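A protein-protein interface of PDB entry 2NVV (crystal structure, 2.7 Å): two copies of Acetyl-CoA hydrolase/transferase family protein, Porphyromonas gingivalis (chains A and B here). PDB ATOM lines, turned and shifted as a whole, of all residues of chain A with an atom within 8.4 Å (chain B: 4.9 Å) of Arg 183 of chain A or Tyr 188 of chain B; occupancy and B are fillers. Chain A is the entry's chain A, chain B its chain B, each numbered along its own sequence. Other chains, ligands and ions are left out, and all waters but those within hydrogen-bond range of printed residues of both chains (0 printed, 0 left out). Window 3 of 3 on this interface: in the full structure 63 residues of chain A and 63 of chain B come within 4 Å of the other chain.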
ATOM      1  N   PRO A 176     -19.841  -1.394   6.243  1.00  0.00           N
ATOM      2  CA  PRO A 176     -19.443  -0.134   6.875  1.00  0.00           C
ATOM      3  C   PRO A 176     -19.046   0.884   5.811  1.00  0.00           C
ATOM      4  O   PRO A 176     -18.849   0.535   4.652  1.00  0.00           O
ATOM      5  CB  PRO A 176     -18.251  -0.549   7.723  1.00  0.00           C
ATOM      6  CG  PRO A 176     -17.580  -1.539   6.826  1.00  0.00           C
ATOM      7  CD  PRO A 176     -18.733  -2.368   6.274  1.00  0.00           C
ATOM      8  N   LEU A 177     -18.945   2.147   6.204  1.00  0.00           N
ATOM      9  CA  LEU A 177     -18.509   3.170   5.270  1.00  0.00           C
ATOM     10  C   LEU A 177     -17.049   2.805   5.006  1.00  0.00           C
ATOM     11  O   LEU A 177     -16.452   2.036   5.756  1.00  0.00           O
ATOM     12  CB  LEU A 177     -18.615   4.556   5.915  1.00  0.00           C
ATOM     13  CG  LEU A 177     -19.881   5.398   5.712  1.00  0.00           C
ATOM     14  CD1 LEU A 177     -21.047   4.537   5.288  1.00  0.00           C
ATOM     15  CD2 LEU A 177     -20.197   6.150   7.015  1.00  0.00           C
ATOM     16  N   ASP A 178     -16.471   3.334   3.939  1.00  0.00           N
ATOM     17  CA  ASP A 178     -15.088   3.028   3.630  1.00  0.00           C
ATOM     18  C   ASP A 178     -14.201   4.232   3.920  1.00  0.00           C
ATOM     19  O   ASP A 178     -14.665   5.372   3.961  1.00  0.00           O
ATOM     20  CB  ASP A 178     -14.972   2.597   2.169  1.00  0.00           C
ATOM     21  CG  ASP A 178     -15.642   1.257   1.904  1.00  0.00           C
ATOM     22  OD1 ASP A 178     -16.224   1.073   0.812  1.00  0.00           O
ATOM     23  OD2 ASP A 178     -15.581   0.382   2.795  1.00  0.00           O
ATOM     24  N   PRO A 179     -12.905   3.996   4.150  1.00  0.00           N
ATOM     25  CA  PRO A 179     -12.035   5.142   4.431  1.00  0.00           C
ATOM     26  C   PRO A 179     -12.116   6.225   3.365  1.00  0.00           C
ATOM     27  O   PRO A 179     -12.339   5.947   2.191  1.00  0.00           O
ATOM     28  CB  PRO A 179     -10.638   4.512   4.557  1.00  0.00           C
ATOM     29  CG  PRO A 179     -10.759   3.179   3.877  1.00  0.00           C
ATOM     30  CD  PRO A 179     -12.154   2.727   4.204  1.00  0.00           C
ATOM     31  N   PRO A 180     -11.909   7.485   3.762  1.00  0.00           N
ATOM     32  CA  PRO A 180     -11.608   7.906   5.132  1.00  0.00           C
ATOM     33  C   PRO A 180     -12.833   8.143   6.016  1.00  0.00           C
ATOM     34  O   PRO A 180     -12.731   8.836   7.023  1.00  0.00           O
ATOM     35  CB  PRO A 180     -10.833   9.189   4.905  1.00  0.00           C
ATOM     36  CG  PRO A 180     -11.617   9.808   3.771  1.00  0.00           C
ATOM     37  CD  PRO A 180     -11.861   8.636   2.838  1.00  0.00           C
ATOM     38  N   ALA A 181     -13.975   7.563   5.659  1.00  0.00           N
ATOM     39  CA  ALA A 181     -15.206   7.774   6.417  1.00  0.00           C
ATOM     40  C   ALA A 181     -15.665   6.638   7.335  1.00  0.00           C
ATOM     41  O   ALA A 181     -16.716   6.726   7.948  1.00  0.00           O
ATOM     42  CB  ALA A 181     -16.326   8.117   5.454  1.00  0.00           C
ATOM     43  N   ARG A 182     -14.876   5.583   7.446  1.00  0.00           N
ATOM     44  CA  ARG A 182     -15.293   4.463   8.265  1.00  0.00           C
ATOM     45  C   ARG A 182     -15.357   4.741   9.754  1.00  0.00           C
ATOM     46  O   ARG A 182     -14.481   5.392  10.315  1.00  0.00           O
ATOM     47  CB  ARG A 182     -14.399   3.251   8.004  1.00  0.00           C
ATOM     48  CG  ARG A 182     -14.917   1.983   8.656  1.00  0.00           C
ATOM     49  CD  ARG A 182     -14.164   0.774   8.156  1.00  0.00           C
ATOM     50  NE  ARG A 182     -14.381   0.522   6.735  1.00  0.00           N
ATOM     51  CZ  ARG A 182     -13.680  -0.356   6.019  1.00  0.00           C
ATOM     52  NH1 ARG A 182     -13.947  -0.522   4.727  1.00  0.00           N
ATOM     53  NH2 ARG A 182     -12.703  -1.063   6.584  1.00  0.00           N
ATOM     54  N   ARG A 183     -16.422   4.249  10.382  1.00  0.00           N
ATOM     55  CA  ARG A 183     -16.634   4.381  11.816  1.00  0.00           C
ATOM     56  C   ARG A 183     -16.320   3.012  12.431  1.00  0.00           C
ATOM     57  O   ARG A 183     -15.924   2.085  11.726  1.00  0.00           O
ATOM     58  CB  ARG A 183     -18.086   4.754  12.107  1.00  0.00           C
ATOM     59  CG  ARG A 183     -18.552   6.022  11.426  1.00  0.00           C
ATOM     60  CD  ARG A 183     -17.761   7.221  11.877  1.00  0.00           C
ATOM     61  NE  ARG A 183     -17.966   7.519  13.291  1.00  0.00           N
ATOM     62  CZ  ARG A 183     -17.322   8.485  13.947  1.00  0.00           C
ATOM     63  NH1 ARG A 183     -16.430   9.237  13.310  1.00  0.00           N
ATOM     64  NH2 ARG A 183     -17.579   8.709  15.230  1.00  0.00           N
ATOM     65  N   GLU A 184     -16.499   2.870  13.736  1.00  0.00           N
ATOM     66  CA  GLU A 184     -16.216   1.590  14.366  1.00  0.00           C
ATOM     67  C   GLU A 184     -17.338   0.596  14.072  1.00  0.00           C
ATOM     68  O   GLU A 184     -18.444   0.986  13.704  1.00  0.00           O
ATOM     69  CB  GLU A 184     -16.041   1.769  15.882  1.00  0.00           C
ATOM     70  CG  GLU A 184     -17.324   1.826  16.713  1.00  0.00           C
ATOM     71  CD  GLU A 184     -18.157   3.075  16.486  1.00  0.00           C
ATOM     72  OE1 GLU A 184     -17.621   4.083  15.968  1.00  0.00           O
ATOM     73  OE2 GLU A 184     -19.354   3.049  16.851  1.00  0.00           O
ATOM     74  N   LEU A 185     -17.037  -0.690  14.211  1.00  0.00           N
ATOM     75  CA  LEU A 185     -18.024  -1.746  14.002  1.00  0.00           C
ATOM     76  C   LEU A 185     -18.532  -2.042  15.415  1.00  0.00           C
ATOM     77  O   LEU A 185     -17.898  -2.762  16.170  1.00  0.00           O
ATOM     78  CB  LEU A 185     -17.344  -2.974  13.403  1.00  0.00           C
ATOM     79  CG  LEU A 185     -16.350  -2.694  12.276  1.00  0.00           C
ATOM     80  CD1 LEU A 185     -15.714  -3.993  11.863  1.00  0.00           C
ATOM     81  CD2 LEU A 185     -17.047  -2.027  11.101  1.00  0.00           C
ATOM     82  N   PRO A 186     -19.694  -1.480  15.778  1.00  0.00           N
ATOM     83  CA  PRO A 186     -20.352  -1.610  17.081  1.00  0.00           C
ATOM     84  C   PRO A 186     -20.737  -2.969  17.676  1.00  0.00           C
ATOM     85  O   PRO A 186     -21.859  -3.137  18.158  1.00  0.00           O
ATOM     86  CB  PRO A 186     -21.555  -0.676  16.947  1.00  0.00           C
ATOM     87  CG  PRO A 186     -21.907  -0.793  15.516  1.00  0.00           C
ATOM     88  CD  PRO A 186     -20.560  -0.746  14.834  1.00  0.00           C
ATOM     89  N   TYR A 188     -19.749  -5.384  20.656  1.00  0.00           N
ATOM     90  CA  TYR A 188     -18.986  -5.512  21.891  1.00  0.00           C
ATOM     91  C   TYR A 188     -19.294  -6.837  22.592  1.00  0.00           C
ATOM     92  O   TYR A 188     -18.675  -7.188  23.598  1.00  0.00           O
ATOM     93  CB  TYR A 188     -19.320  -4.328  22.796  1.00  0.00           C
ATOM     94  CG  TYR A 188     -19.187  -3.006  22.068  1.00  0.00           C
ATOM     95  CD1 TYR A 188     -17.944  -2.400  21.905  1.00  0.00           C
ATOM     96  CD2 TYR A 188     -20.290  -2.415  21.458  1.00  0.00           C
ATOM     97  CE1 TYR A 188     -17.799  -1.238  21.138  1.00  0.00           C
ATOM     98  CE2 TYR A 188     -20.158  -1.261  20.693  1.00  0.00           C
ATOM     99  CZ  TYR A 188     -18.909  -0.681  20.534  1.00  0.00           C
ATOM    100  OH  TYR A 188     -18.772   0.444  19.746  1.00  0.00           O
ATOM    101  N   TYR A 335     -17.718  -9.270   8.831  1.00  0.00           N
ATOM    102  CA  TYR A 335     -17.926  -9.066  10.262  1.00  0.00           C
ATOM    103  C   TYR A 335     -17.619 -10.292  11.111  1.00  0.00           C
ATOM    104  O   TYR A 335     -16.988 -10.173  12.148  1.00  0.00           O
ATOM    105  CB  TYR A 335     -19.349  -8.615  10.530  1.00  0.00           C
ATOM    106  CG  TYR A 335     -19.619  -7.212  10.051  1.00  0.00           C
ATOM    107  CD1 TYR A 335     -19.970  -6.956   8.723  1.00  0.00           C
ATOM    108  CD2 TYR A 335     -19.499  -6.131  10.927  1.00  0.00           C
ATOM    109  CE1 TYR A 335     -20.196  -5.659   8.285  1.00  0.00           C
ATOM    110  CE2 TYR A 335     -19.718  -4.835  10.499  1.00  0.00           C
ATOM    111  CZ  TYR A 335     -20.067  -4.600   9.182  1.00  0.00           C
ATOM    112  OH  TYR A 335     -20.289  -3.303   8.782  1.00  0.00           O
ATOM    113  N   GLU A 340     -10.917  -6.408  14.025  1.00  0.00           N
ATOM    114  CA  GLU A 340     -11.366  -5.461  15.048  1.00  0.00           C
ATOM    115  C   GLU A 340     -12.260  -6.148  16.092  1.00  0.00           C
ATOM    116  O   GLU A 340     -12.038  -6.016  17.298  1.00  0.00           O
ATOM    117  CB  GLU A 340     -12.139  -4.314  14.386  1.00  0.00           C
ATOM    118  CG  GLU A 340     -12.649  -3.238  15.334  1.00  0.00           C
ATOM    119  CD  GLU A 340     -13.425  -2.128  14.628  1.00  0.00           C
ATOM    120  OE1 GLU A 340     -12.988  -1.671  13.557  1.00  0.00           O
ATOM    121  OE2 GLU A 340     -14.469  -1.700  15.153  1.00  0.00           O
ATOM    122  N   ARG A 344     -11.103  -7.255  19.914  1.00  0.00           N
ATOM    123  CA  ARG A 344     -11.833  -6.559  20.968  1.00  0.00           C
ATOM    124  C   ARG A 344     -12.526  -7.539  21.922  1.00  0.00           C
ATOM    125  O   ARG A 344     -12.425  -7.375  23.136  1.00  0.00           O
ATOM    126  CB  ARG A 344     -12.885  -5.629  20.378  1.00  0.00           C
ATOM    127  CG  ARG A 344     -13.753  -4.930  21.431  1.00  0.00           C
ATOM    128  CD  ARG A 344     -14.814  -4.063  20.758  1.00  0.00           C
ATOM    129  NE  ARG A 344     -14.224  -3.149  19.780  1.00  0.00           N
ATOM    130  CZ  ARG A 344     -14.837  -2.736  18.674  1.00  0.00           C
ATOM    131  NH1 ARG A 344     -16.063  -3.152  18.401  1.00  0.00           N
ATOM    132  NH2 ARG A 344     -14.217  -1.916  17.834  1.00  0.00           N
ATOM    133  N   GLU B 184     -14.830   0.107  21.663  1.00  0.00           N
ATOM    134  CA  GLU B 184     -14.059   0.459  20.476  1.00  0.00           C
ATOM    135  C   GLU B 184     -13.010   1.520  20.810  1.00  0.00           C
ATOM    136  O   GLU B 184     -13.116   2.212  21.824  1.00  0.00           O
ATOM    137  CB  GLU B 184     -14.990   0.955  19.356  1.00  0.00           C
ATOM    138  CG  GLU B 184     -15.406   2.429  19.424  1.00  0.00           C
ATOM    139  CD  GLU B 184     -16.328   2.754  20.587  1.00  0.00           C
ATOM    140  OE1 GLU B 184     -16.958   1.831  21.144  1.00  0.00           O
ATOM    141  OE2 GLU B 184     -16.434   3.945  20.939  1.00  0.00           O
ATOM    142  N   PRO B 186     -11.959   4.792  19.828  1.00  0.00           N
ATOM    143  CA  PRO B 186     -12.480   5.986  19.146  1.00  0.00           C
ATOM    144  C   PRO B 186     -11.595   6.891  18.293  1.00  0.00           C
ATOM    145  O   PRO B 186     -11.640   8.106  18.432  1.00  0.00           O
ATOM    146  CB  PRO B 186     -13.185   6.743  20.277  1.00  0.00           C
ATOM    147  CG  PRO B 186     -12.365   6.421  21.462  1.00  0.00           C
ATOM    148  CD  PRO B 186     -12.074   4.940  21.293  1.00  0.00           C
ATOM    149  N   VAL B 187     -10.793   6.315  17.407  1.00  0.00           N
ATOM    150  CA  VAL B 187      -9.991   7.149  16.519  1.00  0.00           C
ATOM    151  C   VAL B 187     -10.473   6.908  15.076  1.00  0.00           C
ATOM    152  O   VAL B 187     -10.343   5.804  14.530  1.00  0.00           O
ATOM    153  CB  VAL B 187      -8.487   6.857  16.661  1.00  0.00           C
ATOM    154  CG1 VAL B 187      -8.260   5.395  16.714  1.00  0.00           C
ATOM    155  CG2 VAL B 187      -7.719   7.460  15.489  1.00  0.00           C
ATOM    156  N   TYR B 188     -11.057   7.945  14.483  1.00  0.00           N
ATOM    157  CA  TYR B 188     -11.613   7.872  13.136  1.00  0.00           C
ATOM    158  C   TYR B 188     -10.820   8.758  12.184  1.00  0.00           C
ATOM    159  O   TYR B 188     -11.042   8.767  10.971  1.00  0.00           O
ATOM    160  CB  TYR B 188     -13.078   8.306  13.189  1.00  0.00           C
ATOM    161  CG  TYR B 188     -13.844   7.556  14.257  1.00  0.00           C
ATOM    162  CD1 TYR B 188     -14.324   6.270  14.022  1.00  0.00           C
ATOM    163  CD2 TYR B 188     -14.012   8.102  15.534  1.00  0.00           C
ATOM    164  CE1 TYR B 188     -14.950   5.542  15.034  1.00  0.00           C
ATOM    165  CE2 TYR B 188     -14.635   7.383  16.547  1.00  0.00           C
ATOM    166  CZ  TYR B 188     -15.101   6.105  16.293  1.00  0.00           C
ATOM    167  OH  TYR B 188     -15.719   5.394  17.293  1.00  0.00           O
ATOM    168  N   THR B 189      -9.882   9.497  12.764  1.00  0.00           N
ATOM    169  CA  THR B 189      -8.997  10.389  12.026  1.00  0.00           C
ATOM    170  C   THR B 189      -7.624  10.233  12.673  1.00  0.00           C
ATOM    171  O   THR B 189      -7.522   9.974  13.874  1.00  0.00           O
ATOM    172  CB  THR B 189      -9.478  11.840  12.148  1.00  0.00           C
ATOM    173  OG1 THR B 189     -10.679  12.000  11.383  1.00  0.00           O
ATOM    174  CG2 THR B 189      -8.436  12.798  11.648  1.00  0.00           C
ATOM    175  N   PRO B 190      -6.547  10.372  11.891  1.00  0.00           N
ATOM    176  CA  PRO B 190      -5.238  10.221  12.525  1.00  0.00           C
ATOM    177  C   PRO B 190      -4.895  11.231  13.638  1.00  0.00           C
ATOM    178  O   PRO B 190      -3.959  11.014  14.401  1.00  0.00           O
ATOM    179  CB  PRO B 190      -4.266  10.269  11.332  1.00  0.00           C
ATOM    180  CG  PRO B 190      -4.997  11.008  10.304  1.00  0.00           C
ATOM    181  CD  PRO B 190      -6.405  10.517  10.434  1.00  0.00           C
ATOM    182  N   ASP B 192      -7.208  12.252  16.053  1.00  0.00           N
ATOM    183  CA  ASP B 192      -8.182  12.169  17.130  1.00  0.00           C
ATOM    184  C   ASP B 192      -7.557  11.815  18.472  1.00  0.00           C
ATOM    185  O   ASP B 192      -6.729  10.919  18.572  1.00  0.00           O
ATOM    186  CB  ASP B 192      -9.274  11.149  16.797  1.00  0.00           C
ATOM    187  CG  ASP B 192     -10.207  11.625  15.703  1.00  0.00           C
ATOM    188  OD1 ASP B 192     -10.115  12.805  15.301  1.00  0.00           O
ATOM    189  OD2 ASP B 192     -11.044  10.816  15.250  1.00  0.00           O
ATOM    190  N   ARG B 344      -9.413   0.616   9.822  1.00  0.00           N
ATOM    191  CA  ARG B 344     -10.513   1.560   9.729  1.00  0.00           C
ATOM    192  C   ARG B 344     -10.130   2.804   8.927  1.00  0.00           C
ATOM    193  O   ARG B 344     -10.883   3.257   8.048  1.00  0.00           O
ATOM    194  CB  ARG B 344     -10.980   1.981  11.119  1.00  0.00           C
ATOM    195  CG  ARG B 344     -12.091   3.032  11.106  1.00  0.00           C
ATOM    196  CD  ARG B 344     -12.457   3.446  12.525  1.00  0.00           C
ATOM    197  NE  ARG B 344     -12.784   2.289  13.359  1.00  0.00           N
ATOM    198  CZ  ARG B 344     -12.578   2.224  14.670  1.00  0.00           C
ATOM    199  NH1 ARG B 344     -12.046   3.247  15.315  1.00  0.00           N
ATOM    200  NH2 ARG B 344     -12.893   1.123  15.335  1.00  0.00           N
ATOM    201  N   LEU B 345      -8.959   3.361   9.227  1.00  0.00           N
ATOM    202  CA  LEU B 345      -8.507   4.563   8.541  1.00  0.00           C
ATOM    203  C   LEU B 345      -8.038   4.292   7.120  1.00  0.00           C
ATOM    204  O   LEU B 345      -7.906   5.215   6.316  1.00  0.00           O
ATOM    205  CB  LEU B 345      -7.373   5.232   9.316  1.00  0.00           C
ATOM    206  CG  LEU B 345      -7.508   5.593  10.801  1.00  0.00           C
ATOM    207  CD1 LEU B 345      -6.280   6.383  11.211  1.00  0.00           C
ATOM    208  CD2 LEU B 345      -8.757   6.405  11.057  1.00  0.00           C
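OH of Tyr 188 of chain B sits at hydrogen-bond distance from OE1 of Glu 184 of chain A. The side-chain hydroxyl (OH) of Tyr 188 of chain A sits at hydrogen-bond distance from the side-chain carboxylate (OE1) of Glu 184 of chain B (2.7 Å). The side-chain carboxylate (OE2) of Glu 340 of chain A is in salt-bridge range of the guanidinium group (NH2) of Arg 344 of chain B (3.2 Å).
The backbone carbonyl oxygen (O) of Leu 177 of chain A sits at hydrogen-bond distance from the guanidinium group (NE) of Arg 182 of chain A, at 2.7 Å. N of Leu 185 of chain A lies within hydrogen-bond range of OE2 of Glu 340 of chain A, 2.9 Å away. The backbone carbonyl oxygen of Leu 185 of chain A lies within hydrogen-bond range of the guanidinium group of Arg 344 of chain A (2.9 Å). The side-chain carboxylate of Glu 340 of chain A lies within salt-bridge range of the guanidinium group of Arg 344 of chain A (2.7 Å). The backbone carbonyl oxygen (O) of Val 187 of chain B lies within hydrogen-bond range of the guanidinium group (NH1) of Arg 344 of chain B. The backbone NH (N) of Tyr 188 of chain B sits at hydrogen-bond distance from the side-chain carboxylate (OD2) of Asp 192 of chain B.
Arg 183 of chain A touches two residues of chain B. Of chain A, only Arg 182 (3.8 Å), Arg 183 (3.2 Å) and Glu 184 (2.7 Å) come within 4 Å of Tyr 188 of chain B. Of the printed residues of chain B, Glu 340 of chain A touches Arg 344 (3.2 Å). Of the printed residues of chain B, Glu 184 of chain A touches Glu 184, Tyr 188 and Arg 344. Of the printed residues of chain A, Leu 345 of chain B touches Pro 179 (3.3 Å). Printed residues of chain B within 4 Å of Pro 179 of chain A: Arg 344 and Leu 345. Of the printed residues of chain A, Arg 344 of chain B touches Pro 179 (3.7 Å), Arg 182 (3.5 Å), Arg 183 (3.5 Å), Glu 184 (3.3 Å) and Glu 340 (3.2 Å). Asp 178 of chain A touches none of the printed residues of chain B. The nearest printed residue of chain B that does not touch Arg 183 of chain A is Asp 192 of chain B (5.9 Å). The nearest residue of chain A that does not touch Tyr 188 of chain B is Pro 180 of chain A (4.3 Å). The nearest printed residue of chain A that does not touch Leu 345 of chain B is Pro 180 of chain A (4.7 Å).
Glu 184 of chain B touches its own counterpart, Glu 184 of chain A. Glu 184 of chain A touches Tyr 188 of chain B, and with the chains exchanged Tyr 188 of chain A touches Glu 184 of chain B. Glu 184 of chain A touches Arg 344 of chain B, and with the chains exchanged Arg 344 of chain A touches Glu 184 of chain B. 4 positions are printed for both chains. Of the 12 pairs that touch across the chains among the printed residues, 5 have their exchanged pair printed and touching as well.
Among the printed residues, pairs that only touch across the chains: Arg 183 of chain A with Tyr 188 of chain B, Glu 184 of chain A with Arg 344 of chain B, Pro 179 of chain A with Leu 345 of chain B, Arg 344 of chain A with Glu 184 of chain B, Glu 184 of chain A with Glu 184 of chain B, Arg 182 of chain A with Arg 344 of chain B, Arg 183 of chain A with Arg 344 of chain B, Pro 179 of chain A with Arg 344 of chain B and Arg 182 of chain A with Tyr 188 of chain B.
Printed residues of chain B that touch a printed residue of chain A: Glu 184, Tyr 188, Arg 344 and Leu 345. Among the printed residues, Asp or Glu carboxylates within 4 Å of a Lys or Arg side-chain nitrogen of the other chain: Glu 340 of chain A with Arg 344 of chain B.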
